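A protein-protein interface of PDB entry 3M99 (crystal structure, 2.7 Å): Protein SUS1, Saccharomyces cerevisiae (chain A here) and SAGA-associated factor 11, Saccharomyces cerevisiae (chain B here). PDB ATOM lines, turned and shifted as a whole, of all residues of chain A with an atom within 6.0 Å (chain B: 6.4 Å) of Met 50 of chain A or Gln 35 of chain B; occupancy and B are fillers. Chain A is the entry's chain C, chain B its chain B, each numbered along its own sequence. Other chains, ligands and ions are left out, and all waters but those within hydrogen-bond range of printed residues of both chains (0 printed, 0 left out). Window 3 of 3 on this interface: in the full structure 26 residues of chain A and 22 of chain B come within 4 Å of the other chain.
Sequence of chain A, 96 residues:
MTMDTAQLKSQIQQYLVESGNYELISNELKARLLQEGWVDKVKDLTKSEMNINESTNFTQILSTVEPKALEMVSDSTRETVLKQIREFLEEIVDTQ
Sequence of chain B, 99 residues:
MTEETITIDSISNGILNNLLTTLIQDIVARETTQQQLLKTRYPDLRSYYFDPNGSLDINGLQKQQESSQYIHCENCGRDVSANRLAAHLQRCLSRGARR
Among the printed residues, merely in contact across the chains: Thr 46 of chain A with Val 28 of chain B (3.5 Å), Thr 46 of chain A with Glu 31 of chain B (3.5 Å), Lys 47 of chain A with Glu 31 of chain B (3.1 Å), Met 50 of chain A with Glu 31 of chain B (3.6 Å), Met 50 of chain A with Thr 32 of chain B (3.7 Å), Met 50 of chain A with Gln 35 of chain B (3.8 Å) and Thr 56 of chain A with Thr 32 of chain B (3.6 Å).
O of Lys 47 of chain A lies close to OD1 of Asn 51 of chain A. O of Met 50 of chain A is in hydrogen-bond range of N of Ser 55 of chain A (3.2 Å).
Hydrophobic or aromatic side chains of chain A within 4 Å of the printed part of chain B: Met 50. Of the 13 printed residues of chain B, 5 touch a printed residue of chain A. Printed residues of chain B that touch a printed residue of chain A: Val 28, Glu 31, Thr 32, Gln 35 and Lys 39. Along chain B the printed residues that touch a printed residue of chain A span positions 28 to 39.
NZ of Lys 39 of chain B is in salt-bridge range of OE2 of Glu 54 of chain A (2.6 Å).
Of the printed residues of chain B, Thr 46 of chain A touches Val 28 (3.5 Å) and Glu 31 (3.5 Å). Ser 48 of chain A touches none of the printed residues of chain B. Of the printed residues of chain B, Glu 54 of chain A touches Lys 39. Of the printed residues of chain B, Thr 56 of chain A touches Thr 32 (3.6 Å). Of the printed residues of chain A, Val 28 of chain B touches Thr 46. Of the printed residues of chain A, Thr 32 of chain B touches Met 50 (3.7 Å) and Thr 56 (3.6 Å). Gln 35 of chain B touches just one residue of chain A: Met 50 (3.8 Å). The nearest residue of chain B that does not touch Met 50 of chain A is Lys 39 of chain B (4.3 Å). The nearest residue of chain A that does not touch Gln 35 of chain B is Thr 56 of chain A (4.1 Å). The nearest printed residue of chain A that does not touch Thr 32 of chain B is Ile 61 of chain A (4.4 Å).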
ATOM      1  N   LEU A  45       8.418  -8.424  24.528  1.00  0.00           N
ATOM      2  CA  LEU A  45       9.005  -8.818  23.253  1.00  0.00           C
ATOM      3  C   LEU A  45       8.204  -8.253  22.096  1.00  0.00           C
ATOM      4  O   LEU A  45       8.763  -7.838  21.080  1.00  0.00           O
ATOM      5  CB  LEU A  45       9.045 -10.339  23.117  1.00  0.00           C
ATOM      6  CG  LEU A  45       9.638 -10.792  21.783  1.00  0.00           C
ATOM      7  CD1 LEU A  45      11.042 -10.219  21.621  1.00  0.00           C
ATOM      8  CD2 LEU A  45       9.644 -12.311  21.663  1.00  0.00           C
ATOM      9  N   THR A  46       6.885  -8.250  22.251  1.00  0.00           N
ATOM     10  CA  THR A  46       6.008  -7.752  21.204  1.00  0.00           C
ATOM     11  C   THR A  46       6.241  -6.257  20.974  1.00  0.00           C
ATOM     12  O   THR A  46       6.313  -5.806  19.833  1.00  0.00           O
ATOM     13  CB  THR A  46       4.515  -8.068  21.504  1.00  0.00           C
ATOM     14  OG1 THR A  46       4.296  -9.479  21.388  1.00  0.00           O
ATOM     15  CG2 THR A  46       3.594  -7.358  20.535  1.00  0.00           C
ATOM     16  N   LYS A  47       6.392  -5.495  22.051  1.00  0.00           N
ATOM     17  CA  LYS A  47       6.574  -4.052  21.925  1.00  0.00           C
ATOM     18  C   LYS A  47       7.944  -3.640  21.347  1.00  0.00           C
ATOM     19  O   LYS A  47       8.088  -2.549  20.790  1.00  0.00           O
ATOM     20  CB  LYS A  47       6.321  -3.371  23.268  1.00  0.00           C
ATOM     21  CG  LYS A  47       4.969  -3.706  23.873  1.00  0.00           C
ATOM     22  CD  LYS A  47       4.975  -3.443  25.372  1.00  0.00           C
ATOM     23  CE  LYS A  47       3.667  -3.849  26.023  1.00  0.00           C
ATOM     24  NZ  LYS A  47       3.849  -4.040  27.488  1.00  0.00           N
ATOM     25  N   SER A  48       8.947  -4.504  21.491  1.00  0.00           N
ATOM     26  CA  SER A  48      10.223  -4.297  20.820  1.00  0.00           C
ATOM     27  C   SER A  48       9.983  -4.265  19.322  1.00  0.00           C
ATOM     28  O   SER A  48      10.263  -3.270  18.656  1.00  0.00           O
ATOM     29  CB  SER A  48      11.198  -5.429  21.141  1.00  0.00           C
ATOM     30  OG  SER A  48      11.834  -5.218  22.384  1.00  0.00           O
ATOM     31  N   GLU A  49       9.450  -5.368  18.805  1.00  0.00           N
ATOM     32  CA  GLU A  49       9.154  -5.493  17.386  1.00  0.00           C
ATOM     33  C   GLU A  49       8.327  -4.319  16.863  1.00  0.00           C
ATOM     34  O   GLU A  49       8.501  -3.904  15.722  1.00  0.00           O
ATOM     35  CB  GLU A  49       8.432  -6.812  17.105  1.00  0.00           C
ATOM     36  CG  GLU A  49       9.057  -8.023  17.788  1.00  0.00           C
ATOM     37  CD  GLU A  49      10.396  -8.421  17.194  1.00  0.00           C
ATOM     38  OE1 GLU A  49      10.520  -8.445  15.949  1.00  0.00           O
ATOM     39  OE2 GLU A  49      11.323  -8.722  17.976  1.00  0.00           O
ATOM     40  N   MET A  50       7.437  -3.780  17.692  1.00  0.00           N
ATOM     41  CA  MET A  50       6.589  -2.660  17.274  1.00  0.00           C
ATOM     42  C   MET A  50       7.309  -1.312  17.211  1.00  0.00           C
ATOM     43  O   MET A  50       7.023  -0.490  16.340  1.00  0.00           O
ATOM     44  CB  MET A  50       5.348  -2.545  18.161  1.00  0.00           C
ATOM     45  CG  MET A  50       4.149  -3.302  17.629  1.00  0.00           C
ATOM     46  SD  MET A  50       2.649  -3.055  18.595  1.00  0.00           S
ATOM     47  CE  MET A  50       3.049  -3.999  20.059  1.00  0.00           C
ATOM     48  N   ASN A  51       8.221  -1.072  18.146  1.00  0.00           N
ATOM     49  CA  ASN A  51       8.992   0.160  18.121  1.00  0.00           C
ATOM     50  C   ASN A  51      10.189  -0.004  17.194  1.00  0.00           C
ATOM     51  O   ASN A  51      10.534   0.906  16.439  1.00  0.00           O
ATOM     52  CB  ASN A  51       9.433   0.570  19.529  1.00  0.00           C
ATOM     53  CG  ASN A  51       8.254   0.873  20.451  1.00  0.00           C
ATOM     54  OD1 ASN A  51       7.240   0.166  20.440  1.00  0.00           O
ATOM     55  ND2 ASN A  51       8.386   1.924  21.260  1.00  0.00           N
ATOM     56  N   ILE A  52      10.794  -1.189  17.236  1.00  0.00           N
ATOM     57  CA  ILE A  52      11.960  -1.514  16.416  1.00  0.00           C
ATOM     58  C   ILE A  52      11.626  -1.661  14.929  1.00  0.00           C
ATOM     59  O   ILE A  52      12.013  -0.814  14.124  1.00  0.00           O
ATOM     60  CB  ILE A  52      12.680  -2.769  16.950  1.00  0.00           C
ATOM     61  CG1 ILE A  52      13.383  -2.428  18.274  1.00  0.00           C
ATOM     62  CG2 ILE A  52      13.646  -3.322  15.914  1.00  0.00           C
ATOM     63  CD1 ILE A  52      14.075  -3.599  18.960  1.00  0.00           C
ATOM     64  N   ASN A  53      10.910  -2.721  14.559  1.00  0.00           N
ATOM     65  CA  ASN A  53      10.473  -2.886  13.169  1.00  0.00           C
ATOM     66  C   ASN A  53       9.505  -1.791  12.739  1.00  0.00           C
ATOM     67  O   ASN A  53       9.013  -1.795  11.612  1.00  0.00           O
ATOM     68  CB  ASN A  53       9.817  -4.251  12.946  1.00  0.00           C
ATOM     69  CG  ASN A  53      10.803  -5.397  13.027  1.00  0.00           C
ATOM     70  OD1 ASN A  53      11.274  -5.753  14.109  1.00  0.00           O
ATOM     71  ND2 ASN A  53      11.109  -5.995  11.881  1.00  0.00           N
ATOM     72  N   GLU A  54       9.230  -0.865  13.650  1.00  0.00           N
ATOM     73  CA  GLU A  54       8.317   0.241  13.388  1.00  0.00           C
ATOM     74  C   GLU A  54       7.086  -0.204  12.589  1.00  0.00           C
ATOM     75  O   GLU A  54       6.961   0.110  11.403  1.00  0.00           O
ATOM     76  CB  GLU A  54       9.044   1.380  12.668  1.00  0.00           C
ATOM     77  CG  GLU A  54       8.350   2.732  12.774  1.00  0.00           C
ATOM     78  CD  GLU A  54       6.849   2.599  12.963  1.00  0.00           C
ATOM     79  OE1 GLU A  54       6.095   2.709  11.963  1.00  0.00           O
ATOM     80  OE2 GLU A  54       6.430   2.362  14.119  1.00  0.00           O
ATOM     81  N   SER A  55       6.182  -0.920  13.255  1.00  0.00           N
ATOM     82  CA  SER A  55       4.976  -1.467  12.628  1.00  0.00           C
ATOM     83  C   SER A  55       3.983  -1.984  13.677  1.00  0.00           C
ATOM     84  O   SER A  55       4.389  -2.478  14.734  1.00  0.00           O
ATOM     85  CB  SER A  55       5.350  -2.603  11.668  1.00  0.00           C
ATOM     86  OG  SER A  55       4.213  -3.359  11.275  1.00  0.00           O
ATOM     87  N   THR A  56       2.688  -1.876  13.383  1.00  0.00           N
ATOM     88  CA  THR A  56       1.653  -2.413  14.272  1.00  0.00           C
ATOM     89  C   THR A  56       0.774  -3.444  13.563  1.00  0.00           C
ATOM     90  O   THR A  56      -0.378  -3.667  13.947  1.00  0.00           O
ATOM     91  CB  THR A  56       0.756  -1.304  14.857  1.00  0.00           C
ATOM     92  OG1 THR A  56       0.275  -0.465  13.801  1.00  0.00           O
ATOM     93  CG2 THR A  56       1.528  -0.459  15.859  1.00  0.00           C
ATOM     94  N   ASN A  57       1.329  -4.068  12.529  1.00  0.00           N
ATOM     95  CA  ASN A  57       0.607  -5.063  11.748  1.00  0.00           C
ATOM     96  C   ASN A  57       0.662  -6.429  12.425  1.00  0.00           C
ATOM     97  O   ASN A  57       1.739  -6.955  12.698  1.00  0.00           O
ATOM     98  CB  ASN A  57       1.178  -5.127  10.324  1.00  0.00           C
ATOM     99  CG  ASN A  57       0.485  -6.162   9.453  1.00  0.00           C
ATOM    100  OD1 ASN A  57       0.774  -7.358   9.534  1.00  0.00           O
ATOM    101  ND2 ASN A  57      -0.419  -5.701   8.596  1.00  0.00           N
ATOM    102  N   ILE A  61       4.067  -8.599  12.925  1.00  0.00           N
ATOM    103  CA  ILE A  61       4.679  -8.723  14.242  1.00  0.00           C
ATOM    104  C   ILE A  61       4.608 -10.157  14.784  1.00  0.00           C
ATOM    105  O   ILE A  61       5.514 -10.605  15.491  1.00  0.00           O
ATOM    106  CB  ILE A  61       4.046  -7.731  15.251  1.00  0.00           C
ATOM    107  CG1 ILE A  61       4.156  -6.289  14.729  1.00  0.00           C
ATOM    108  CG2 ILE A  61       4.682  -7.876  16.633  1.00  0.00           C
ATOM    109  CD1 ILE A  61       5.574  -5.811  14.509  1.00  0.00           C
ATOM    110  N   VAL B  28      -0.276 -11.033  21.562  1.00  0.00           N
ATOM    111  CA  VAL B  28       0.183 -10.090  20.537  1.00  0.00           C
ATOM    112  C   VAL B  28      -0.961  -9.256  19.975  1.00  0.00           C
ATOM    113  O   VAL B  28      -0.828  -8.049  19.767  1.00  0.00           O
ATOM    114  CB  VAL B  28       0.869 -10.829  19.371  1.00  0.00           C
ATOM    115  CG1 VAL B  28       1.327  -9.844  18.302  1.00  0.00           C
ATOM    116  CG2 VAL B  28       2.039 -11.664  19.881  1.00  0.00           C
ATOM    117  N   ARG B  30      -3.483  -8.100  21.294  1.00  0.00           N
ATOM    118  CA  ARG B  30      -3.939  -7.046  22.184  1.00  0.00           C
ATOM    119  C   ARG B  30      -2.904  -5.939  22.241  1.00  0.00           C
ATOM    120  O   ARG B  30      -3.229  -4.781  22.477  1.00  0.00           O
ATOM    121  CB  ARG B  30      -4.186  -7.598  23.585  1.00  0.00           C
ATOM    122  CG  ARG B  30      -5.250  -8.675  23.682  1.00  0.00           C
ATOM    123  CD  ARG B  30      -5.367  -9.140  25.129  1.00  0.00           C
ATOM    124  NE  ARG B  30      -6.212 -10.318  25.302  1.00  0.00           N
ATOM    125  CZ  ARG B  30      -7.413 -10.291  25.866  1.00  0.00           C
ATOM    126  NH1 ARG B  30      -7.905  -9.140  26.302  1.00  0.00           N
ATOM    127  NH2 ARG B  30      -8.123 -11.406  25.993  1.00  0.00           N
ATOM    128  N   GLU B  31      -1.648  -6.305  22.029  1.00  0.00           N
ATOM    129  CA  GLU B  31      -0.576  -5.322  21.988  1.00  0.00           C
ATOM    130  C   GLU B  31      -0.659  -4.468  20.723  1.00  0.00           C
ATOM    131  O   GLU B  31      -0.686  -3.234  20.800  1.00  0.00           O
ATOM    132  CB  GLU B  31       0.787  -6.008  22.098  1.00  0.00           C
ATOM    133  CG  GLU B  31       0.988  -6.731  23.413  1.00  0.00           C
ATOM    134  CD  GLU B  31       0.633  -5.854  24.590  1.00  0.00           C
ATOM    135  OE1 GLU B  31       1.078  -4.685  24.601  1.00  0.00           O
ATOM    136  OE2 GLU B  31      -0.095  -6.324  25.496  1.00  0.00           O
ATOM    137  N   THR B  32      -0.709  -5.122  19.564  1.00  0.00           N
ATOM    138  CA  THR B  32      -0.760  -4.395  18.304  1.00  0.00           C
ATOM    139  C   THR B  32      -2.017  -3.535  18.245  1.00  0.00           C
ATOM    140  O   THR B  32      -2.017  -2.454  17.656  1.00  0.00           O
ATOM    141  CB  THR B  32      -0.699  -5.336  17.083  1.00  0.00           C
ATOM    142  OG1 THR B  32      -1.935  -6.041  16.947  1.00  0.00           O
ATOM    143  CG2 THR B  32       0.429  -6.341  17.238  1.00  0.00           C
ATOM    144  N   THR B  33      -3.078  -4.022  18.880  1.00  0.00           N
ATOM    145  CA  THR B  33      -4.363  -3.334  18.919  1.00  0.00           C
ATOM    146  C   THR B  33      -4.282  -2.030  19.693  1.00  0.00           C
ATOM    147  O   THR B  33      -4.835  -1.010  19.273  1.00  0.00           O
ATOM    148  CB  THR B  33      -5.429  -4.213  19.593  1.00  0.00           C
ATOM    149  OG1 THR B  33      -5.922  -5.181  18.658  1.00  0.00           O
ATOM    150  CG2 THR B  33      -6.582  -3.359  20.093  1.00  0.00           C
ATOM    151  N   GLN B  34      -3.589  -2.076  20.830  1.00  0.00           N
ATOM    152  CA  GLN B  34      -3.519  -0.944  21.745  1.00  0.00           C
ATOM    153  C   GLN B  34      -2.584   0.153  21.260  1.00  0.00           C
ATOM    154  O   GLN B  34      -2.897   1.334  21.401  1.00  0.00           O
ATOM    155  CB  GLN B  34      -3.053  -1.401  23.118  1.00  0.00           C
ATOM    156  CG  GLN B  34      -3.925  -2.429  23.787  1.00  0.00           C
ATOM    157  CD  GLN B  34      -3.315  -2.893  25.087  1.00  0.00           C
ATOM    158  OE1 GLN B  34      -2.883  -2.075  25.905  1.00  0.00           O
ATOM    159  NE2 GLN B  34      -3.258  -4.206  25.286  1.00  0.00           N
ATOM    160  N   GLN B  35      -1.428  -0.233  20.723  1.00  0.00           N
ATOM    161  CA  GLN B  35      -0.501   0.749  20.156  1.00  0.00           C
ATOM    162  C   GLN B  35      -1.112   1.390  18.925  1.00  0.00           C
ATOM    163  O   GLN B  35      -1.020   2.603  18.742  1.00  0.00           O
ATOM    164  CB  GLN B  35       0.848   0.096  19.848  1.00  0.00           C
ATOM    165  CG  GLN B  35       1.986   0.573  20.736  1.00  0.00           C
ATOM    166  CD  GLN B  35       2.348   2.026  20.489  1.00  0.00           C
ATOM    167  OE1 GLN B  35       1.688   2.717  19.714  1.00  0.00           O
ATOM    168  NE2 GLN B  35       3.389   2.497  21.164  1.00  0.00           N
ATOM    169  N   GLN B  36      -1.732   0.553  18.093  1.00  0.00           N
ATOM    170  CA  GLN B  36      -2.440   0.996  16.906  1.00  0.00           C
ATOM    171  C   GLN B  36      -3.458   2.073  17.256  1.00  0.00           C
ATOM    172  O   GLN B  36      -3.673   3.001  16.483  1.00  0.00           O
ATOM    173  CB  GLN B  36      -3.136  -0.189  16.230  1.00  0.00           C
ATOM    174  CG  GLN B  36      -4.016   0.193  15.056  1.00  0.00           C
ATOM    175  CD  GLN B  36      -4.534  -1.012  14.291  1.00  0.00           C
ATOM    176  OE1 GLN B  36      -5.476  -1.682  14.716  1.00  0.00           O
ATOM    177  NE2 GLN B  36      -3.928  -1.283  13.144  1.00  0.00           N
ATOM    178  N   LEU B  37      -4.083   1.952  18.423  1.00  0.00           N
ATOM    179  CA  LEU B  37      -5.037   2.956  18.873  1.00  0.00           C
ATOM    180  C   LEU B  37      -4.318   4.199  19.388  1.00  0.00           C
ATOM    181  O   LEU B  37      -4.712   5.321  19.075  1.00  0.00           O
ATOM    182  CB  LEU B  37      -5.951   2.392  19.961  1.00  0.00           C
ATOM    183  CG  LEU B  37      -6.784   3.447  20.694  1.00  0.00           C
ATOM    184  CD1 LEU B  37      -7.712   4.161  19.718  1.00  0.00           C
ATOM    185  CD2 LEU B  37      -7.568   2.837  21.854  1.00  0.00           C
ATOM    186  N   LEU B  38      -3.269   3.993  20.183  1.00  0.00           N
ATOM    187  CA  LEU B  38      -2.477   5.089  20.741  1.00  0.00           C
ATOM    188  C   LEU B  38      -1.917   5.990  19.664  1.00  0.00           C
ATOM    189  O   LEU B  38      -1.980   7.217  19.769  1.00  0.00           O
ATOM    190  CB  LEU B  38      -1.304   4.541  21.536  1.00  0.00           C
ATOM    191  CG  LEU B  38      -1.652   4.080  22.937  1.00  0.00           C
ATOM    192  CD1 LEU B  38      -0.412   3.481  23.565  1.00  0.00           C
ATOM    193  CD2 LEU B  38      -2.182   5.266  23.729  1.00  0.00           C
ATOM    194  N   LYS B  39      -1.340   5.361  18.644  1.00  0.00           N
ATOM    195  CA  LYS B  39      -0.718   6.077  17.547  1.00  0.00           C
ATOM    196  C   LYS B  39      -1.752   6.896  16.792  1.00  0.00           C
ATOM    197  O   LYS B  39      -1.535   8.073  16.527  1.00  0.00           O
ATOM    198  CB  LYS B  39       0.005   5.109  16.609  1.00  0.00           C
ATOM    199  CG  LYS B  39       1.278   4.502  17.199  1.00  0.00           C
ATOM    200  CD  LYS B  39       2.125   3.838  16.109  1.00  0.00           C
ATOM    201  CE  LYS B  39       3.526   3.476  16.611  1.00  0.00           C
ATOM    202  NZ  LYS B  39       4.307   2.707  15.593  1.00  0.00           N
ATOM    203  N   THR B  40      -2.882   6.281  16.462  1.00  0.00           N
ATOM    204  CA  THR B  40      -3.944   6.987  15.750  1.00  0.00           C
ATOM    205  C   THR B  40      -4.580   8.084  16.603  1.00  0.00           C
ATOM    206  O   THR B  40      -4.880   9.171  16.110  1.00  0.00           O
ATOM    207  CB  THR B  40      -5.046   6.027  15.281  1.00  0.00           C
ATOM    208  OG1 THR B  40      -4.471   4.992  14.473  1.00  0.00           O
ATOM    209  CG2 THR B  40      -6.089   6.778  14.474  1.00  0.00           C
ATOM    210  N   LEU B  45       2.598  11.549  20.130  1.00  0.00           N
ATOM    211  CA  LEU B  45       2.810  10.816  21.377  1.00  0.00           C
ATOM    212  C   LEU B  45       4.125  11.126  22.095  1.00  0.00           C
ATOM    213  O   LEU B  45       5.209  10.799  21.605  1.00  0.00           O
ATOM    214  CB  LEU B  45       2.696   9.306  21.158  1.00  0.00           C
ATOM    215  CG  LEU B  45       2.917   8.488  22.434  1.00  0.00           C
ATOM    216  CD1 LEU B  45       1.902   8.882  23.504  1.00  0.00           C
ATOM    217  CD2 LEU B  45       2.869   6.992  22.155  1.00  0.00           C
